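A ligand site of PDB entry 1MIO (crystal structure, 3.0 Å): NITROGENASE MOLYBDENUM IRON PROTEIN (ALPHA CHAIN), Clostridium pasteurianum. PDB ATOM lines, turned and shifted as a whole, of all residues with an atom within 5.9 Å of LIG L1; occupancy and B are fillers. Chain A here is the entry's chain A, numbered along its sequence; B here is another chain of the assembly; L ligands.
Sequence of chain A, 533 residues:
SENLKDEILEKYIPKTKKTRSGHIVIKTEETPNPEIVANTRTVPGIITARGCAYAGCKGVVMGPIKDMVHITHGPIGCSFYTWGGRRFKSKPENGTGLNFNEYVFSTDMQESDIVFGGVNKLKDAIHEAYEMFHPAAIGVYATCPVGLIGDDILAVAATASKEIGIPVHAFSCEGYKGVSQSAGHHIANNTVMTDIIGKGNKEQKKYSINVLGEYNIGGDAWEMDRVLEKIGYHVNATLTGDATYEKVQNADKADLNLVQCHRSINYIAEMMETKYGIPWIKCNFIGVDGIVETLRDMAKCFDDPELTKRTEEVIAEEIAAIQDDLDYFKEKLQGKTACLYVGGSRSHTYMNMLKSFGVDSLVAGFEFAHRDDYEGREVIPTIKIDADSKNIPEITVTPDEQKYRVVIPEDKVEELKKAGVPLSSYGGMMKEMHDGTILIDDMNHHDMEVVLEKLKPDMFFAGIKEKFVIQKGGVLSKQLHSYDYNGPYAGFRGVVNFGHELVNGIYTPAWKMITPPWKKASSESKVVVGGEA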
ATOM      1  N   GLY A  51     -28.252 -15.169  -1.697  1.00  0.00           N
ATOM      2  CA  GLY A  51     -28.908 -15.853  -0.610  1.00  0.00           C
ATOM      3  C   GLY A  51     -28.377 -15.408   0.742  1.00  0.00           C
ATOM      4  O   GLY A  51     -27.932 -14.291   0.914  1.00  0.00           O
ATOM      5  N   ALA A  55     -28.195 -20.615   3.832  1.00  0.00           N
ATOM      6  CA  ALA A  55     -28.246 -21.342   2.581  1.00  0.00           C
ATOM      7  C   ALA A  55     -26.911 -22.009   2.320  1.00  0.00           C
ATOM      8  O   ALA A  55     -26.886 -23.160   1.928  1.00  0.00           O
ATOM      9  CB  ALA A  55     -28.524 -20.408   1.430  1.00  0.00           C
ATOM     10  N   GLY A  56     -25.801 -21.299   2.596  1.00  0.00           N
ATOM     11  CA  GLY A  56     -24.444 -21.743   2.414  1.00  0.00           C
ATOM     12  C   GLY A  56     -24.009 -22.671   3.515  1.00  0.00           C
ATOM     13  O   GLY A  56     -23.245 -23.581   3.231  1.00  0.00           O
ATOM     14  N   GLY A  59     -27.819 -25.415   3.844  1.00  0.00           N
ATOM     15  CA  GLY A  59     -28.282 -25.996   2.591  1.00  0.00           C
ATOM     16  C   GLY A  59     -27.236 -26.529   1.648  1.00  0.00           C
ATOM     17  O   GLY A  59     -27.434 -27.558   1.015  1.00  0.00           O
ATOM     18  N   VAL A  60     -26.129 -25.790   1.504  1.00  0.00           N
ATOM     19  CA  VAL A  60     -25.041 -26.144   0.585  1.00  0.00           C
ATOM     20  C   VAL A  60     -24.033 -27.138   1.103  1.00  0.00           C
ATOM     21  O   VAL A  60     -23.926 -28.241   0.567  1.00  0.00           O
ATOM     22  CB  VAL A  60     -24.268 -24.835   0.108  1.00  0.00           C
ATOM     23  CG1 VAL A  60     -22.993 -25.179  -0.668  1.00  0.00           C
ATOM     24  CG2 VAL A  60     -25.122 -24.026  -0.831  1.00  0.00           C
ATOM     25  N   GLY A  85     -34.583 -28.933  -3.236  1.00  0.00           N
ATOM     26  CA  GLY A  85     -34.283 -28.077  -4.381  1.00  0.00           C
ATOM     27  C   GLY A  85     -32.828 -28.116  -4.908  1.00  0.00           C
ATOM     28  O   GLY A  85     -32.587 -27.870  -6.097  1.00  0.00           O
ATOM     29  N   ARG A  86     -31.856 -28.319  -3.968  1.00  0.00           N
ATOM     30  CA  ARG A  86     -30.412 -28.424  -4.227  1.00  0.00           C
ATOM     31  C   ARG A  86     -30.199 -29.916  -4.547  1.00  0.00           C
ATOM     32  O   ARG A  86     -30.465 -30.779  -3.709  1.00  0.00           O
ATOM     33  CB  ARG A  86     -29.606 -27.975  -2.976  1.00  0.00           C
ATOM     34  CG  ARG A  86     -28.459 -26.947  -3.115  1.00  0.00           C
ATOM     35  CD  ARG A  86     -27.240 -27.342  -3.940  1.00  0.00           C
ATOM     36  NE  ARG A  86     -26.322 -28.113  -3.119  1.00  0.00           N
ATOM     37  CZ  ARG A  86     -25.055 -27.764  -2.791  1.00  0.00           C
ATOM     38  NH1 ARG A  86     -24.479 -26.645  -3.211  1.00  0.00           N
ATOM     39  NH2 ARG A  86     -24.359 -28.568  -1.997  1.00  0.00           N
ATOM     40  N   ARG A  87     -29.720 -30.259  -5.735  1.00  0.00           N
ATOM     41  CA  ARG A  87     -29.741 -31.622  -6.236  1.00  0.00           C
ATOM     42  C   ARG A  87     -28.640 -32.601  -5.963  1.00  0.00           C
ATOM     43  O   ARG A  87     -28.162 -33.334  -6.847  1.00  0.00           O
ATOM     44  CB  ARG A  87     -29.968 -31.505  -7.739  1.00  0.00           C
ATOM     45  CG  ARG A  87     -31.335 -31.640  -8.353  1.00  0.00           C
ATOM     46  CD  ARG A  87     -31.093 -31.212  -9.779  1.00  0.00           C
ATOM     47  NE  ARG A  87     -30.036 -31.906 -10.504  1.00  0.00           N
ATOM     48  CZ  ARG A  87     -30.270 -33.032 -11.175  1.00  0.00           C
ATOM     49  NH1 ARG A  87     -31.456 -33.600 -11.222  1.00  0.00           N
ATOM     50  NH2 ARG A  87     -29.341 -33.555 -11.949  1.00  0.00           N
ATOM     51  N   GLN A 181     -24.138 -16.277   0.598  1.00  0.00           N
ATOM     52  CA  GLN A 181     -23.907 -17.659   0.983  1.00  0.00           C
ATOM     53  C   GLN A 181     -22.469 -17.963   1.333  1.00  0.00           C
ATOM     54  O   GLN A 181     -22.247 -19.060   1.833  1.00  0.00           O
ATOM     55  CB  GLN A 181     -24.274 -18.648  -0.100  1.00  0.00           C
ATOM     56  CG  GLN A 181     -25.717 -18.741  -0.532  1.00  0.00           C
ATOM     57  CD  GLN A 181     -25.979 -17.932  -1.785  1.00  0.00           C
ATOM     58  OE1 GLN A 181     -26.013 -16.710  -1.733  1.00  0.00           O
ATOM     59  NE2 GLN A 181     -26.125 -18.543  -2.951  1.00  0.00           N
ATOM     60  N   ILE A 217     -24.041 -33.125  -7.494  1.00  0.00           N
ATOM     61  CA  ILE A 217     -25.283 -32.683  -8.102  1.00  0.00           C
ATOM     62  C   ILE A 217     -25.556 -33.387  -9.426  1.00  0.00           C
ATOM     63  O   ILE A 217     -24.860 -33.328 -10.455  1.00  0.00           O
ATOM     64  CB  ILE A 217     -25.217 -31.133  -8.217  1.00  0.00           C
ATOM     65  CG1 ILE A 217     -25.237 -30.570  -6.789  1.00  0.00           C
ATOM     66  CG2 ILE A 217     -26.340 -30.558  -9.079  1.00  0.00           C
ATOM     67  CD1 ILE A 217     -25.168 -29.056  -6.729  1.00  0.00           C
ATOM     68  N   ARG A 346     -18.804 -22.125 -10.817  1.00  0.00           N
ATOM     69  CA  ARG A 346     -19.289 -22.563 -12.120  1.00  0.00           C
ATOM     70  C   ARG A 346     -19.164 -21.672 -13.322  1.00  0.00           C
ATOM     71  O   ARG A 346     -18.823 -22.192 -14.388  1.00  0.00           O
ATOM     72  CB  ARG A 346     -20.734 -22.988 -12.006  1.00  0.00           C
ATOM     73  CG  ARG A 346     -20.558 -24.252 -11.244  1.00  0.00           C
ATOM     74  CD  ARG A 346     -21.766 -25.085 -11.024  1.00  0.00           C
ATOM     75  NE  ARG A 346     -21.393 -26.188 -10.168  1.00  0.00           N
ATOM     76  CZ  ARG A 346     -22.303 -27.027  -9.667  1.00  0.00           C
ATOM     77  NH1 ARG A 346     -23.613 -26.909  -9.925  1.00  0.00           N
ATOM     78  NH2 ARG A 346     -21.890 -27.979  -8.828  1.00  0.00           N
ATOM     79  N   GLU A 367     -22.238 -14.485  -8.194  1.00  0.00           N
ATOM     80  CA  GLU A 367     -23.144 -14.062  -7.159  1.00  0.00           C
ATOM     81  C   GLU A 367     -22.411 -13.528  -5.921  1.00  0.00           C
ATOM     82  O   GLU A 367     -22.388 -12.341  -5.631  1.00  0.00           O
ATOM     83  CB  GLU A 367     -23.989 -15.302  -6.873  1.00  0.00           C
ATOM     84  CG  GLU A 367     -25.370 -15.087  -6.320  1.00  0.00           C
ATOM     85  CD  GLU A 367     -26.323 -16.127  -6.879  1.00  0.00           C
ATOM     86  OE1 GLU A 367     -26.540 -16.140  -8.091  1.00  0.00           O
ATOM     87  OE2 GLU A 367     -26.836 -16.930  -6.105  1.00  0.00           O
ATOM     88  N   ALA A 462     -27.444 -19.211 -16.089  1.00  0.00           N
ATOM     89  CA  ALA A 462     -27.834 -18.628 -14.810  1.00  0.00           C
ATOM     90  C   ALA A 462     -28.619 -19.696 -14.021  1.00  0.00           C
ATOM     91  O   ALA A 462     -28.251 -20.887 -14.017  1.00  0.00           O
ATOM     92  CB  ALA A 462     -28.695 -17.345 -15.068  1.00  0.00           C
ATOM     93  N   GLY A 463     -29.729 -19.314 -13.369  1.00  0.00           N
ATOM     94  CA  GLY A 463     -30.464 -20.202 -12.490  1.00  0.00           C
ATOM     95  C   GLY A 463     -31.920 -19.884 -12.517  1.00  0.00           C
ATOM     96  O   GLY A 463     -32.295 -18.966 -13.222  1.00  0.00           O
ATOM     97  N   ILE A 464     -32.681 -20.564 -11.661  1.00  0.00           N
ATOM     98  CA  ILE A 464     -34.130 -20.555 -11.686  1.00  0.00           C
ATOM     99  C   ILE A 464     -34.816 -19.209 -11.777  1.00  0.00           C
ATOM    100  O   ILE A 464     -35.666 -19.094 -12.655  1.00  0.00           O
ATOM    101  CB  ILE A 464     -34.666 -21.406 -10.436  1.00  0.00           C
ATOM    102  CG1 ILE A 464     -36.110 -21.762 -10.690  1.00  0.00           C
ATOM    103  CG2 ILE A 464     -34.655 -20.688  -9.124  1.00  0.00           C
ATOM    104  CD1 ILE A 464     -36.244 -22.900 -11.729  1.00  0.00           C
ATOM    105  N   LYS A 465     -34.441 -18.166 -11.037  1.00  0.00           N
ATOM    106  CA  LYS A 465     -35.161 -16.925 -11.229  1.00  0.00           C
ATOM    107  C   LYS A 465     -34.740 -16.186 -12.503  1.00  0.00           C
ATOM    108  O   LYS A 465     -35.565 -15.462 -13.084  1.00  0.00           O
ATOM    109  CB  LYS A 465     -34.991 -15.966 -10.058  1.00  0.00           C
ATOM    110  CG  LYS A 465     -35.400 -16.516  -8.717  1.00  0.00           C
ATOM    111  CD  LYS A 465     -34.130 -16.870  -7.977  1.00  0.00           C
ATOM    112  CE  LYS A 465     -33.525 -15.649  -7.282  1.00  0.00           C
ATOM    113  NZ  LYS A 465     -32.183 -15.878  -6.844  1.00  0.00           N
ATOM    114  N   GLU A 466     -33.487 -16.337 -12.991  1.00  0.00           N
ATOM    115  CA  GLU A 466     -33.040 -15.632 -14.188  1.00  0.00           C
ATOM    116  C   GLU A 466     -33.569 -16.322 -15.448  1.00  0.00           C
ATOM    117  O   GLU A 466     -34.057 -15.691 -16.388  1.00  0.00           O
ATOM    118  CB  GLU A 466     -31.521 -15.587 -14.249  1.00  0.00           C
ATOM    119  CG  GLU A 466     -30.827 -14.766 -13.183  1.00  0.00           C
ATOM    120  CD  GLU A 466     -30.294 -15.471 -11.911  1.00  0.00           C
ATOM    121  OE1 GLU A 466     -31.025 -16.292 -11.344  1.00  0.00           O
ATOM    122  OE2 GLU A 466     -29.153 -15.188 -11.487  1.00  0.00           O
ATOM    123  N   GLN A 479     -29.706 -24.005 -16.925  1.00  0.00           N
ATOM    124  CA  GLN A 479     -29.304 -23.752 -15.554  1.00  0.00           C
ATOM    125  C   GLN A 479     -28.126 -24.571 -15.157  1.00  0.00           C
ATOM    126  O   GLN A 479     -28.133 -25.798 -15.181  1.00  0.00           O
ATOM    127  CB  GLN A 479     -30.365 -24.077 -14.588  1.00  0.00           C
ATOM    128  CG  GLN A 479     -31.710 -23.488 -14.893  1.00  0.00           C
ATOM    129  CD  GLN A 479     -32.643 -24.012 -13.855  1.00  0.00           C
ATOM    130  OE1 GLN A 479     -32.245 -24.017 -12.681  1.00  0.00           O
ATOM    131  NE2 GLN A 479     -33.823 -24.509 -14.193  1.00  0.00           N
ATOM    132  N   HIS A 481     -26.678 -24.347 -12.008  1.00  0.00           N
ATOM    133  CA  HIS A 481     -26.785 -24.795 -10.638  1.00  0.00           C
ATOM    134  C   HIS A 481     -27.464 -26.165 -10.633  1.00  0.00           C
ATOM    135  O   HIS A 481     -26.843 -27.184 -10.333  1.00  0.00           O
ATOM    136  CB  HIS A 481     -27.645 -23.839  -9.836  1.00  0.00           C
ATOM    137  CG  HIS A 481     -27.052 -22.497  -9.421  1.00  0.00           C
ATOM    138  ND1 HIS A 481     -26.896 -22.068  -8.175  1.00  0.00           N
ATOM    139  CD2 HIS A 481     -26.912 -21.385 -10.216  1.00  0.00           C
ATOM    140  CE1 HIS A 481     -26.674 -20.769  -8.194  1.00  0.00           C
ATOM    141  NE2 HIS A 481     -26.690 -20.369  -9.424  1.00  0.00           N
ATOM    142  N   SER A 482     -28.742 -26.213 -11.007  1.00  0.00           N
ATOM    143  CA  SER A 482     -29.570 -27.415 -11.049  1.00  0.00           C
ATOM    144  C   SER A 482     -29.390 -28.342 -12.243  1.00  0.00           C
ATOM    145  O   SER A 482     -30.134 -29.339 -12.343  1.00  0.00           O
ATOM    146  CB  SER A 482     -31.038 -27.077 -11.060  1.00  0.00           C
ATOM    147  OG  SER A 482     -31.418 -26.654 -12.363  1.00  0.00           O
ATOM    148  N   TYR B  51     -35.395 -17.472  -1.821  1.00  0.00           N
ATOM    149  CA  TYR B  51     -36.105 -18.723  -1.601  1.00  0.00           C
ATOM    150  C   TYR B  51     -37.600 -18.654  -1.978  1.00  0.00           C
ATOM    151  O   TYR B  51     -38.131 -19.459  -2.771  1.00  0.00           O
ATOM    152  CB  TYR B  51     -35.893 -19.112  -0.096  1.00  0.00           C
ATOM    153  CG  TYR B  51     -34.659 -19.968   0.388  1.00  0.00           C
ATOM    154  CD1 TYR B  51     -33.717 -20.543  -0.473  1.00  0.00           C
ATOM    155  CD2 TYR B  51     -34.487 -20.199   1.761  1.00  0.00           C
ATOM    156  CE1 TYR B  51     -32.648 -21.298   0.029  1.00  0.00           C
ATOM    157  CE2 TYR B  51     -33.425 -20.948   2.249  1.00  0.00           C
ATOM    158  CZ  TYR B  51     -32.521 -21.501   1.383  1.00  0.00           C
ATOM    159  OH  TYR B  51     -31.473 -22.287   1.847  1.00  0.00           O
ATOM    160  N   THR B  54     -38.235 -18.234  -5.545  1.00  0.00           N
ATOM    161  CA  THR B  54     -37.957 -19.465  -6.222  1.00  0.00           C
ATOM    162  C   THR B  54     -39.130 -20.432  -6.119  1.00  0.00           C
ATOM    163  O   THR B  54     -39.418 -21.004  -7.158  1.00  0.00           O
ATOM    164  CB  THR B  54     -36.643 -20.010  -5.644  1.00  0.00           C
ATOM    165  OG1 THR B  54     -35.616 -19.283  -6.297  1.00  0.00           O
ATOM    166  CG2 THR B  54     -36.366 -21.458  -5.900  1.00  0.00           C
HETATM  167  C1  LIG L   1     -28.635 -21.648  -2.928  1.00  0.00           C
HETATM  168  C2  LIG L   1     -29.433 -22.418  -3.982  1.00  0.00           C
HETATM  169  C3  LIG L   1     -28.805 -22.594  -5.383  1.00  0.00           C
HETATM  170  C4  LIG L   1     -29.674 -21.718  -6.332  1.00  0.00           C
HETATM  171  C5  LIG L   1     -30.645 -22.339  -7.322  1.00  0.00           C
HETATM  172  C6  LIG L   1     -30.680 -21.762  -8.732  1.00  0.00           C
HETATM  173  C7  LIG L   1     -28.715 -24.071  -5.771  1.00  0.00           C
HETATM  174  O1  LIG L   1     -28.506 -22.088  -1.706  1.00  0.00           O
HETATM  175  O2  LIG L   1     -28.193 -20.461  -3.178  1.00  0.00           O
HETATM  176  O3  LIG L   1     -31.014 -20.507  -8.911  1.00  0.00           O
HETATM  177  O4  LIG L   1     -30.702 -22.573  -9.752  1.00  0.00           O
HETATM  178  O5  LIG L   1     -27.450 -24.540  -6.264  1.00  0.00           O
HETATM  179  O6  LIG L   1     -29.635 -24.839  -5.609  1.00  0.00           O
HETATM  180  O7  LIG L   1     -27.479 -22.062  -5.367  1.00  0.00           O
HETATM  181 FE1  LG2 L   2     -19.261 -23.886  -4.879  1.00  0.00          FE
HETATM  182 FE2  LG2 L   2     -21.482 -22.903  -3.900  1.00  0.00          FE
HETATM  183 FE3  LG2 L   2     -21.474 -25.315  -5.290  1.00  0.00          FE
HETATM  184 FE4  LG2 L   2     -20.789 -22.831  -6.769  1.00  0.00          FE
HETATM  185 FE5  LG2 L   2     -23.260 -22.591  -7.273  1.00  0.00          FE
HETATM  186 FE6  LG2 L   2     -24.026 -22.475  -4.562  1.00  0.00          FE
HETATM  187 FE7  LG2 L   2     -23.870 -24.904  -5.799  1.00  0.00          FE
HETATM  188 MO1  LG2 L   2     -25.869 -23.026  -6.489  1.00  0.00          MO
HETATM  189  S1  LG2 L   2     -19.898 -21.688  -5.022  1.00  0.00           S
HETATM  190  S2  LG2 L   2     -19.850 -24.965  -6.850  1.00  0.00           S
HETATM  191  S3  LG2 L   2     -21.562 -21.913  -8.679  1.00  0.00           S
HETATM  192  S4  LG2 L   2     -20.511 -24.875  -3.232  1.00  0.00           S
HETATM  193  S5  LG2 L   2     -24.620 -21.041  -6.196  1.00  0.00           S
HETATM  194  S6  LG2 L   2     -23.047 -21.767  -2.667  1.00  0.00           S
HETATM  195  S7  LG2 L   2     -25.577 -24.123  -4.445  1.00  0.00           S
HETATM  196  S8  LG2 L   2     -24.561 -24.359  -7.899  1.00  0.00           S
HETATM  197  S9  LG2 L   2     -23.060 -26.970  -5.442  1.00  0.00           S
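The side-chain amide nitrogen (NE2) of Gln 181 is in hydrogen-bond range of an oxygen (O2) of LIG L1, at 2.8 Å.
N of Ile 464 lies within hydrogen-bond range of O3 of LIG L1.
ND1 of His 481 binds MO1 of LG2 L2 (2.2 Å).
The guanidinium group (NH1) of Arg 86 lies close to a sulfur (S9) of LG2 L2.
N of Arg 346 lies close to S3 of LG2 L2.
A sulfur (S8) of LG2 L2 sits close to the guanidinium group (NH1) of Arg 346, 3.4 Å away.
O7 of LIG L1 is bound to MO1 of LG2 L2.
The side-chain amide oxygen (OE1) of Gln 181 sits at hydrogen-bond distance from the backbone NH (N) of Gly 51 of chain A (2.7 Å).
The backbone carbonyl oxygen (O) of His 481 is in hydrogen-bond range of the guanidinium group (NH1) of Arg 346, at 3.3 Å.
The backbone carbonyl oxygen (O) of Val 60 lies within hydrogen-bond range of the guanidinium group (NH2) of Arg 86.
The backbone carbonyl oxygen (O) of Ala 55 lies within hydrogen-bond range of the backbone NH (N) of Val 60, at 2.8 Å.
The side-chain amide oxygen of Gln 479 lies within hydrogen-bond range of the side-chain hydroxyl of Ser 482, 2.8 Å away.
ND1 of His 481 lies close to O7 of LIG L1, at 2.9 Å.
CB of Ala 55 touches O1 of LIG L1 (3.6 Å).
Val 60 touches LIG L1 (CG2 to O1, 3.997 Å).
Arg 86 touches LIG L1.
CA of Gly 463 touches O4 of LIG L1 (3.6 Å).
Gln 479 touches LIG L1 (OE1 to O4, 3.6 Å).
The nearest printed residue that does not touch LIG L1 is Gly 85 (4.3 Å).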
